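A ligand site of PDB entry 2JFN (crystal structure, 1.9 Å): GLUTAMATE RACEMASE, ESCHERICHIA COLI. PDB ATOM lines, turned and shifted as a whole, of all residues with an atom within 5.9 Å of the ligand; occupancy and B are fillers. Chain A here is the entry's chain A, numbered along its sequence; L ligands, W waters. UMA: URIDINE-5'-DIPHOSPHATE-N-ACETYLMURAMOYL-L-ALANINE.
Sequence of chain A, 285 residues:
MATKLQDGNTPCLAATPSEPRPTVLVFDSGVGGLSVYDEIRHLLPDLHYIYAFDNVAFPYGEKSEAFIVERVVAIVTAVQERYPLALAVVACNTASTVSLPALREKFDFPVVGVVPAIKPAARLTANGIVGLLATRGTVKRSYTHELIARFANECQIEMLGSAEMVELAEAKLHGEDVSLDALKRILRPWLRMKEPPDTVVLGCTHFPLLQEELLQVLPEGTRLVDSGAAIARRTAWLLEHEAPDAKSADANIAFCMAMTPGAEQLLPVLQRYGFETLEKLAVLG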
ATOM      1  N   LEU A 100      -9.518   2.051   5.780  1.00  0.00           N
ATOM      2  CA  LEU A 100     -10.644   1.603   4.955  1.00  0.00           C
ATOM      3  C   LEU A 100     -10.855   0.084   4.835  1.00  0.00           C
ATOM      4  O   LEU A 100     -11.968  -0.410   5.048  1.00  0.00           O
ATOM      5  CB  LEU A 100     -10.567   2.249   3.571  1.00  0.00           C
ATOM      6  CG  LEU A 100     -10.682   3.774   3.549  1.00  0.00           C
ATOM      7  CD1 LEU A 100     -10.726   4.263   2.107  1.00  0.00           C
ATOM      8  CD2 LEU A 100     -11.955   4.216   4.281  1.00  0.00           C
ATOM      9  N   ARG A 104     -14.240  -1.615   6.256  1.00  0.00           N
ATOM     10  CA  ARG A 104     -15.168  -2.208   5.315  1.00  0.00           C
ATOM     11  C   ARG A 104     -15.376  -3.688   5.577  1.00  0.00           C
ATOM     12  O   ARG A 104     -16.403  -4.249   5.206  1.00  0.00           O
ATOM     13  CB  ARG A 104     -14.690  -1.970   3.888  1.00  0.00           C
ATOM     14  CG  ARG A 104     -14.915  -0.528   3.448  1.00  0.00           C
ATOM     15  CD  ARG A 104     -14.192  -0.163   2.149  1.00  0.00           C
ATOM     16  NE  ARG A 104     -14.508   1.222   1.779  1.00  0.00           N
ATOM     17  CZ  ARG A 104     -13.790   1.971   0.952  1.00  0.00           C
ATOM     18  NH1 ARG A 104     -12.701   1.496   0.376  1.00  0.00           N
ATOM     19  NH2 ARG A 104     -14.171   3.219   0.706  1.00  0.00           N
ATOM     20  N   VAL A 111     -18.577   2.800   3.742  1.00  0.00           N
ATOM     21  CA  VAL A 111     -17.597   3.655   4.383  1.00  0.00           C
ATOM     22  C   VAL A 111     -16.943   4.512   3.312  1.00  0.00           C
ATOM     23  O   VAL A 111     -16.474   3.998   2.308  1.00  0.00           O
ATOM     24  CB  VAL A 111     -16.509   2.834   5.110  1.00  0.00           C
ATOM     25  CG1 VAL A 111     -15.513   3.773   5.803  1.00  0.00           C
ATOM     26  CG2 VAL A 111     -17.161   1.891   6.140  1.00  0.00           C
ATOM     27  N   VAL A 112     -16.921   5.825   3.540  1.00  0.00           N
ATOM     28  CA  VAL A 112     -16.308   6.741   2.592  1.00  0.00           C
ATOM     29  C   VAL A 112     -14.946   7.166   3.104  1.00  0.00           C
ATOM     30  O   VAL A 112     -14.784   7.446   4.287  1.00  0.00           O
ATOM     31  CB  VAL A 112     -17.198   7.990   2.384  1.00  0.00           C
ATOM     32  CG1 VAL A 112     -16.512   8.991   1.455  1.00  0.00           C
ATOM     33  CG2 VAL A 112     -18.515   7.580   1.788  1.00  0.00           C
ATOM     34  N   GLY A 113     -13.968   7.177   2.209  1.00  0.00           N
ATOM     35  CA  GLY A 113     -12.630   7.580   2.582  1.00  0.00           C
ATOM     36  C   GLY A 113     -12.255   8.867   1.872  1.00  0.00           C
ATOM     37  O   GLY A 113     -13.013   9.383   1.058  1.00  0.00           O
ATOM     38  N   VAL A 114     -11.067   9.378   2.193  1.00  0.00           N
ATOM     39  CA  VAL A 114     -10.581  10.617   1.582  1.00  0.00           C
ATOM     40  C   VAL A 114      -9.124  10.528   1.164  1.00  0.00           C
ATOM     41  O   VAL A 114      -8.275  10.036   1.913  1.00  0.00           O
ATOM     42  CB  VAL A 114     -10.686  11.802   2.551  1.00  0.00           C
ATOM     43  CG1 VAL A 114     -12.128  12.004   2.993  1.00  0.00           C
ATOM     44  CG2 VAL A 114      -9.758  11.574   3.730  1.00  0.00           C
ATOM     45  N   VAL A 115      -8.848  10.984  -0.049  1.00  0.00           N
ATOM     46  CA  VAL A 115      -7.491  11.004  -0.568  1.00  0.00           C
ATOM     47  C   VAL A 115      -7.331  12.397  -1.162  1.00  0.00           C
ATOM     48  O   VAL A 115      -8.303  12.995  -1.632  1.00  0.00           O
ATOM     49  CB  VAL A 115      -7.269   9.941  -1.664  1.00  0.00           C
ATOM     50  CG1 VAL A 115      -7.310   8.545  -1.054  1.00  0.00           C
ATOM     51  CG2 VAL A 115      -8.324  10.065  -2.743  1.00  0.00           C
ATOM     52  N   PRO A 116      -6.109  12.954  -1.136  1.00  0.00           N
ATOM     53  CA  PRO A 116      -5.885  14.297  -1.694  1.00  0.00           C
ATOM     54  C   PRO A 116      -6.433  14.387  -3.108  1.00  0.00           C
ATOM     55  O   PRO A 116      -6.230  13.477  -3.919  1.00  0.00           O
ATOM     56  CB  PRO A 116      -4.371  14.437  -1.638  1.00  0.00           C
ATOM     57  CG  PRO A 116      -4.016  13.652  -0.372  1.00  0.00           C
ATOM     58  CD  PRO A 116      -4.882  12.413  -0.519  1.00  0.00           C
ATOM     59  N   ALA A 117      -7.119  15.490  -3.416  1.00  0.00           N
ATOM     60  CA  ALA A 117      -7.729  15.713  -4.734  1.00  0.00           C
ATOM     61  C   ALA A 117      -6.736  16.016  -5.852  1.00  0.00           C
ATOM     62  O   ALA A 117      -6.906  16.963  -6.614  1.00  0.00           O
ATOM     63  CB  ALA A 117      -8.751  16.844  -4.636  1.00  0.00           C
ATOM     64  N   ILE A 118      -5.698  15.187  -5.952  1.00  0.00           N
ATOM     65  CA  ILE A 118      -4.684  15.385  -6.978  1.00  0.00           C
ATOM     66  C   ILE A 118      -5.232  15.209  -8.376  1.00  0.00           C
ATOM     67  O   ILE A 118      -4.904  15.981  -9.277  1.00  0.00           O
ATOM     68  CB  ILE A 118      -3.514  14.394  -6.768  1.00  0.00           C
ATOM     69  CG1 ILE A 118      -2.790  14.753  -5.474  1.00  0.00           C
ATOM     70  CG2 ILE A 118      -2.565  14.446  -7.966  1.00  0.00           C
ATOM     71  CD1 ILE A 118      -1.721  13.769  -5.072  1.00  0.00           C
ATOM     72  N   LYS A 119      -6.087  14.206  -8.568  1.00  0.00           N
ATOM     73  CA  LYS A 119      -6.670  13.933  -9.883  1.00  0.00           C
ATOM     74  C   LYS A 119      -7.360  15.150 -10.519  1.00  0.00           C
ATOM     75  O   LYS A 119      -7.008  15.548 -11.620  1.00  0.00           O
ATOM     76  CB  LYS A 119      -7.637  12.745  -9.786  1.00  0.00           C
ATOM     77  CG  LYS A 119      -8.186  12.315 -11.149  1.00  0.00           C
ATOM     78  CD  LYS A 119      -9.026  11.058 -11.047  1.00  0.00           C
ATOM     79  CE  LYS A 119      -9.578  10.690 -12.407  1.00  0.00           C
ATOM     80  NZ  LYS A 119     -10.608   9.620 -12.294  1.00  0.00           N
ATOM     81  N   PRO A 120      -8.363  15.745  -9.835  1.00  0.00           N
ATOM     82  CA  PRO A 120      -8.981  16.906 -10.488  1.00  0.00           C
ATOM     83  C   PRO A 120      -8.049  18.112 -10.602  1.00  0.00           C
ATOM     84  O   PRO A 120      -8.147  18.874 -11.564  1.00  0.00           O
ATOM     85  CB  PRO A 120     -10.200  17.188  -9.591  1.00  0.00           C
ATOM     86  CG  PRO A 120      -9.788  16.653  -8.252  1.00  0.00           C
ATOM     87  CD  PRO A 120      -9.096  15.361  -8.619  1.00  0.00           C
ATOM     88  N   TYR A 143       1.218   5.702  -0.134  1.00  0.00           N
ATOM     89  CA  TYR A 143      -0.089   5.872  -0.745  1.00  0.00           C
ATOM     90  C   TYR A 143      -0.129   7.208  -1.481  1.00  0.00           C
ATOM     91  O   TYR A 143      -0.721   7.325  -2.557  1.00  0.00           O
ATOM     92  CB  TYR A 143      -1.183   5.834   0.328  1.00  0.00           C
ATOM     93  CG  TYR A 143      -2.604   5.764  -0.193  1.00  0.00           C
ATOM     94  CD1 TYR A 143      -3.144   6.815  -0.947  1.00  0.00           C
ATOM     95  CD2 TYR A 143      -3.417   4.667   0.077  1.00  0.00           C
ATOM     96  CE1 TYR A 143      -4.461   6.750  -1.414  1.00  0.00           C
ATOM     97  CE2 TYR A 143      -4.737   4.599  -0.377  1.00  0.00           C
ATOM     98  CZ  TYR A 143      -5.253   5.644  -1.128  1.00  0.00           C
ATOM     99  OH  TYR A 143      -6.544   5.591  -1.586  1.00  0.00           O
ATOM    100  N   LEU A 147      -0.253   8.034  -5.711  1.00  0.00           N
ATOM    101  CA  LEU A 147      -1.339   8.796  -6.306  1.00  0.00           C
ATOM    102  C   LEU A 147      -0.786   9.927  -7.162  1.00  0.00           C
ATOM    103  O   LEU A 147      -1.330  10.254  -8.223  1.00  0.00           O
ATOM    104  CB  LEU A 147      -2.247   9.372  -5.208  1.00  0.00           C
ATOM    105  CG  LEU A 147      -3.510  10.114  -5.649  1.00  0.00           C
ATOM    106  CD1 LEU A 147      -4.431   9.175  -6.402  1.00  0.00           C
ATOM    107  CD2 LEU A 147      -4.218  10.677  -4.424  1.00  0.00           C
ATOM    108  N   ARG A 150       0.092   8.384 -10.412  1.00  0.00           N
ATOM    109  CA  ARG A 150      -1.042   7.805 -11.121  1.00  0.00           C
ATOM    110  C   ARG A 150      -1.920   8.802 -11.879  1.00  0.00           C
ATOM    111  O   ARG A 150      -2.268   8.574 -13.040  1.00  0.00           O
ATOM    112  CB  ARG A 150      -1.908   6.998 -10.154  1.00  0.00           C
ATOM    113  CG  ARG A 150      -3.069   6.276 -10.814  1.00  0.00           C
ATOM    114  CD  ARG A 150      -3.834   5.357  -9.845  1.00  0.00           C
ATOM    115  NE  ARG A 150      -3.043   4.209  -9.393  1.00  0.00           N
ATOM    116  CZ  ARG A 150      -2.150   4.259  -8.407  1.00  0.00           C
ATOM    117  NH1 ARG A 150      -1.925   5.388  -7.756  1.00  0.00           N
ATOM    118  NH2 ARG A 150      -1.484   3.157  -8.073  1.00  0.00           N
ATOM    119  N   PHE A 151      -2.291   9.908 -11.238  1.00  0.00           N
ATOM    120  CA  PHE A 151      -3.154  10.899 -11.896  1.00  0.00           C
ATOM    121  C   PHE A 151      -2.512  12.259 -12.136  1.00  0.00           C
ATOM    122  O   PHE A 151      -3.196  13.208 -12.537  1.00  0.00           O
ATOM    123  CB  PHE A 151      -4.450  11.097 -11.109  1.00  0.00           C
ATOM    124  CG  PHE A 151      -5.288   9.844 -10.983  1.00  0.00           C
ATOM    125  CD1 PHE A 151      -5.184   9.044  -9.858  1.00  0.00           C
ATOM    126  CD2 PHE A 151      -6.161   9.482 -11.993  1.00  0.00           C
ATOM    127  CE1 PHE A 151      -5.948   7.877  -9.750  1.00  0.00           C
ATOM    128  CE2 PHE A 151      -6.936   8.320 -11.893  1.00  0.00           C
ATOM    129  CZ  PHE A 151      -6.823   7.523 -10.765  1.00  0.00           C
ATOM    130  N   ASP A 226     -10.131  20.856  -2.940  1.00  0.00           N
ATOM    131  CA  ASP A 226     -10.231  19.864  -1.886  1.00  0.00           C
ATOM    132  C   ASP A 226     -11.246  18.803  -2.273  1.00  0.00           C
ATOM    133  O   ASP A 226     -11.826  18.850  -3.367  1.00  0.00           O
ATOM    134  CB  ASP A 226     -10.540  20.495  -0.518  1.00  0.00           C
ATOM    135  CG  ASP A 226     -11.872  21.207  -0.478  1.00  0.00           C
ATOM    136  OD1 ASP A 226     -12.906  20.593  -0.799  1.00  0.00           O
ATOM    137  OD2 ASP A 226     -11.889  22.406  -0.097  1.00  0.00           O
ATOM    138  N   SER A 227     -11.470  17.857  -1.374  1.00  0.00           N
ATOM    139  CA  SER A 227     -12.374  16.739  -1.620  1.00  0.00           C
ATOM    140  C   SER A 227     -13.811  16.875  -1.115  1.00  0.00           C
ATOM    141  O   SER A 227     -14.648  15.999  -1.378  1.00  0.00           O
ATOM    142  CB  SER A 227     -11.762  15.481  -1.005  1.00  0.00           C
ATOM    143  OG  SER A 227     -10.487  15.225  -1.558  1.00  0.00           O
ATOM    144  N   ALA A 230     -16.970  16.574  -3.524  1.00  0.00           N
ATOM    145  CA  ALA A 230     -16.952  15.238  -4.120  1.00  0.00           C
ATOM    146  C   ALA A 230     -17.344  14.165  -3.106  1.00  0.00           C
ATOM    147  O   ALA A 230     -17.946  13.150  -3.469  1.00  0.00           O
ATOM    148  CB  ALA A 230     -15.576  14.935  -4.682  1.00  0.00           C
ATOM    149  N   ILE A 231     -16.986  14.391  -1.838  1.00  0.00           N
ATOM    150  CA  ILE A 231     -17.304  13.453  -0.768  1.00  0.00           C
ATOM    151  C   ILE A 231     -18.811  13.498  -0.555  1.00  0.00           C
ATOM    152  O   ILE A 231     -19.463  12.474  -0.349  1.00  0.00           O
ATOM    153  CB  ILE A 231     -16.626  13.839   0.563  1.00  0.00           C
ATOM    154  CG1 ILE A 231     -15.109  13.821   0.390  1.00  0.00           C
ATOM    155  CG2 ILE A 231     -17.070  12.895   1.681  1.00  0.00           C
ATOM    156  CD1 ILE A 231     -14.577  12.469   0.032  1.00  0.00           C
ATOM    157  N   ARG A 233     -21.107  14.313  -2.765  1.00  0.00           N
ATOM    158  CA  ARG A 233     -21.735  13.586  -3.874  1.00  0.00           C
ATOM    159  C   ARG A 233     -21.612  12.080  -3.694  1.00  0.00           C
ATOM    160  O   ARG A 233     -22.569  11.350  -3.937  1.00  0.00           O
ATOM    161  CB  ARG A 233     -21.114  14.015  -5.212  1.00  0.00           C
ATOM    162  CG  ARG A 233     -21.450  15.443  -5.641  1.00  0.00           C
ATOM    163  CD  ARG A 233     -21.056  15.686  -7.091  1.00  0.00           C
ATOM    164  NE  ARG A 233     -19.608  15.612  -7.296  1.00  0.00           N
ATOM    165  CZ  ARG A 233     -18.775  16.624  -7.083  1.00  0.00           C
ATOM    166  NH1 ARG A 233     -19.244  17.783  -6.649  1.00  0.00           N
ATOM    167  NH2 ARG A 233     -17.472  16.467  -7.260  1.00  0.00           N
ATOM    168  N   ARG A 234     -20.447  11.606  -3.273  1.00  0.00           N
ATOM    169  CA  ARG A 234     -20.249  10.168  -3.064  1.00  0.00           C
ATOM    170  C   ARG A 234     -21.152   9.668  -1.942  1.00  0.00           C
ATOM    171  O   ARG A 234     -21.676   8.546  -2.004  1.00  0.00           O
ATOM    172  CB  ARG A 234     -18.785   9.882  -2.719  1.00  0.00           C
ATOM    173  CG  ARG A 234     -18.494   8.409  -2.441  1.00  0.00           C
ATOM    174  CD  ARG A 234     -18.860   7.500  -3.612  1.00  0.00           C
ATOM    175  NE  ARG A 234     -18.381   6.144  -3.394  1.00  0.00           N
ATOM    176  CZ  ARG A 234     -18.592   5.123  -4.220  1.00  0.00           C
ATOM    177  NH1 ARG A 234     -19.288   5.313  -5.340  1.00  0.00           N
ATOM    178  NH2 ARG A 234     -18.108   3.922  -3.932  1.00  0.00           N
HETATM  179  N1  UMA L   1     -12.770  11.899  -3.284  1.00  0.00           N
HETATM  180  C2  UMA L   1     -12.385  11.118  -2.079  1.00  0.00           C
HETATM  181  N3  UMA L   1     -13.288  10.131  -1.703  1.00  0.00           N
HETATM  182  C4  UMA L   1     -14.492   9.826  -2.357  1.00  0.00           C
HETATM  183  C5  UMA L   1     -14.819  10.669  -3.576  1.00  0.00           C
HETATM  184  C6  UMA L   1     -13.965  11.642  -3.958  1.00  0.00           C
HETATM  185  O2  UMA L   1     -11.362  11.304  -1.447  1.00  0.00           O
HETATM  186  O4  UMA L   1     -15.201   8.926  -1.922  1.00  0.00           O
HETATM  187  C1B UMA L   1     -11.801  12.980  -3.700  1.00  0.00           C
HETATM  188  C2B UMA L   1     -10.675  12.404  -4.541  1.00  0.00           C
HETATM  189  O2' UMA L   1      -9.348  12.977  -4.239  1.00  0.00           O
HETATM  190  C3B UMA L   1     -11.042  12.590  -5.970  1.00  0.00           C
HETATM  191  C4B UMA L   1     -11.774  13.907  -5.852  1.00  0.00           C
HETATM  192  O4B UMA L   1     -12.362  13.939  -4.554  1.00  0.00           O
HETATM  193  O3B UMA L   1      -9.753  12.628  -6.648  1.00  0.00           O
HETATM  194  C5B UMA L   1     -12.860  14.105  -6.824  1.00  0.00           C
HETATM  195  O5B UMA L   1     -13.664  12.979  -6.886  1.00  0.00           O
HETATM  196  PA  UMA L   1     -14.811  12.765  -7.960  1.00  0.00           P
HETATM  197  O1A UMA L   1     -15.657  11.724  -7.385  1.00  0.00           O
HETATM  198  O2A UMA L   1     -15.448  14.016  -8.220  1.00  0.00           O
HETATM  199  O3A UMA L   1     -13.999  12.172  -9.226  1.00  0.00           O
HETATM  200  PB  UMA L   1     -12.497  11.644  -9.423  1.00  0.00           P
HETATM  201  O1B UMA L   1     -11.520  12.693  -9.214  1.00  0.00           O
HETATM  202  O2B UMA L   1     -12.461  10.913 -10.697  1.00  0.00           O
HETATM  203  O1' UMA L   1     -12.449  10.499  -8.257  1.00  0.00           O
HETATM  204  C1' UMA L   1     -12.463   9.079  -8.449  1.00  0.00           C
HETATM  205  C2' UMA L   1     -13.289   8.383  -7.394  1.00  0.00           C
HETATM  206  N2' UMA L   1     -14.706   8.810  -7.436  1.00  0.00           N
HETATM  207  C7' UMA L   1     -15.689   7.968  -7.810  1.00  0.00           C
HETATM  208  O7' UMA L   1     -15.493   6.769  -7.980  1.00  0.00           O
HETATM  209  C8' UMA L   1     -17.076   8.539  -8.013  1.00  0.00           C
HETATM  210  C3' UMA L   1     -12.648   8.664  -6.027  1.00  0.00           C
HETATM  211  O3' UMA L   1     -13.360   7.933  -4.968  1.00  0.00           O
HETATM  212  C4' UMA L   1     -11.164   8.258  -6.010  1.00  0.00           C
HETATM  213  O4' UMA L   1     -10.566   8.543  -4.757  1.00  0.00           O
HETATM  214  C5' UMA L   1     -10.405   8.975  -7.125  1.00  0.00           C
HETATM  215  O5' UMA L   1     -11.076   8.669  -8.407  1.00  0.00           O
HETATM  216  C6' UMA L   1      -8.964   8.536  -7.277  1.00  0.00           C
HETATM  217  O6' UMA L   1      -8.899   7.123  -7.443  1.00  0.00           O
HETATM  218  C18 UMA L   1     -13.705   6.521  -4.916  1.00  0.00           C
HETATM  219  C19 UMA L   1     -12.743   5.695  -4.141  1.00  0.00           C
HETATM  220  O18 UMA L   1     -12.548   4.525  -4.415  1.00  0.00           O
HETATM  221  C20 UMA L   1     -15.189   6.412  -4.519  1.00  0.00           C
HETATM  222  N4  UMA L   1     -12.114   6.333  -3.134  1.00  0.00           N
HETATM  223  C21 UMA L   1     -11.239   5.714  -2.140  1.00  0.00           C
HETATM  224  C22 UMA L   1     -11.832   4.460  -1.427  1.00  0.00           C
HETATM  225  O19 UMA L   1     -13.072   4.409  -1.294  1.00  0.00           O
HETATM  226  O20 UMA L   1     -11.055   3.551  -1.048  1.00  0.00           O
HETATM  227  C23 UMA L   1     -10.856   6.758  -1.082  1.00  0.00           C
HETATM  228  O   HOH W   1     -17.761  11.594  -5.630  1.00  0.00           O
HETATM  229  O   HOH W   2      -7.191  12.453  -6.320  1.00  0.00           O
HETATM  230  O   HOH W   3      -9.179   4.167  -5.764  1.00  0.00           O
HETATM  231  O   HOH W   4     -10.812   7.360 -11.034  1.00  0.00           O
HETATM  232  O   HOH W   5      -6.772   5.071  -7.730  1.00  0.00           O
HETATM  233  O   HOH W   6     -18.483  13.042  -8.631  1.00  0.00           O
HETATM  234  O   HOH W   7     -13.672   5.553  -9.711  1.00  0.00           O
HETATM  235  O   HOH W   8      -8.457   3.994  -0.213  1.00  0.00           O
HETATM  236  O   HOH W   9     -14.626   6.572  -0.490  1.00  0.00           O
HETATM  237  O   HOH W  10      -8.552   6.691  -4.396  1.00  0.00           O
HETATM  238  O   HOH W  11     -11.212  14.245 -11.297  1.00  0.00           O
HETATM  239  O   HOH W  12     -15.369   2.695  -2.669  1.00  0.00           O
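The guanidinium group of Arg 104 is in salt-bridge range of an oxygen (O19) of the ligand. NZ of Lys 119 is in salt-bridge range of O2B of the ligand (2.8 Å). The backbone NH of Val 115 lies within hydrogen-bond range of an oxygen (O2) of the ligand (2.9 Å). O2' of the ligand lies within hydrogen-bond range of O of Val 115 (2.8 Å). N3 of the ligand sits at hydrogen-bond distance from O of Gly 113, at 2.9 Å. An oxygen (O2') of the ligand lies within hydrogen-bond range of the backbone carbonyl oxygen (O) of Pro 116 (3.2 Å). The backbone NH (N) of Ala 117 lies close to an oxygen (O2') of the ligand (3.5 Å). The guanidinium group (NH2) of Arg 233 is in salt-bridge range of an oxygen (O2A) of the ligand.
Water W2 lies within hydrogen-bond range of O3B of the ligand (2.6 Å), O of Pro 116 (2.8 Å), N of Lys 119 (3.1 Å) and N of Ile 118 (3.1 Å). Water W1 bridges the backbone carbonyl oxygen of Ala 230 and an oxygen (O1A) of the ligand. Water W8 bridges O20 of the ligand (2.8 Å) and OH of Tyr 143 (2.8 Å). Water W9 bridges an oxygen (O19) of the ligand and the backbone NH (N) of Gly 113. Water W4 bridges the side-chain amino group of Lys 119 and an oxygen (O5') of the ligand. Water W6 bridges NE of Arg 233 (3.1 Å) and O2A of the ligand (3.2 Å).
CD1 of Leu 100 touches O20 of the ligand, 3.3 Å away. Val 112 touches the ligand (CG1 to O4, 3.6 Å). CA of Val 114 touches O2 of the ligand, 3.2 Å away. Pro 120 touches the ligand (CD to O3B, 3.4 Å). Phe 151 touches the ligand. OG of Ser 227 touches C1B of the ligand, 3.4 Å away. CB of Ala 230 touches O4B of the ligand, 3.4 Å away. Ile 231 touches the ligand. Arg 234 touches the ligand. 16 residues have an atom within 4 Å of the ligand: Leu 100, Arg 104, Val 112, Gly 113, Val 114, Val 115, Pro 116, Ala 117, Lys 119, Pro 120, Phe 151, Ser 227, Ala 230, Ile 231, Arg 233 and Arg 234.
The backbone carbonyl oxygen (O) of Val 111 sits at hydrogen-bond distance from the guanidinium group (NH2) of Arg 104, at 2.9 Å. The backbone carbonyl oxygen of Val 115 sits at hydrogen-bond distance from the side-chain hydroxyl of Ser 227 (3.1 Å).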
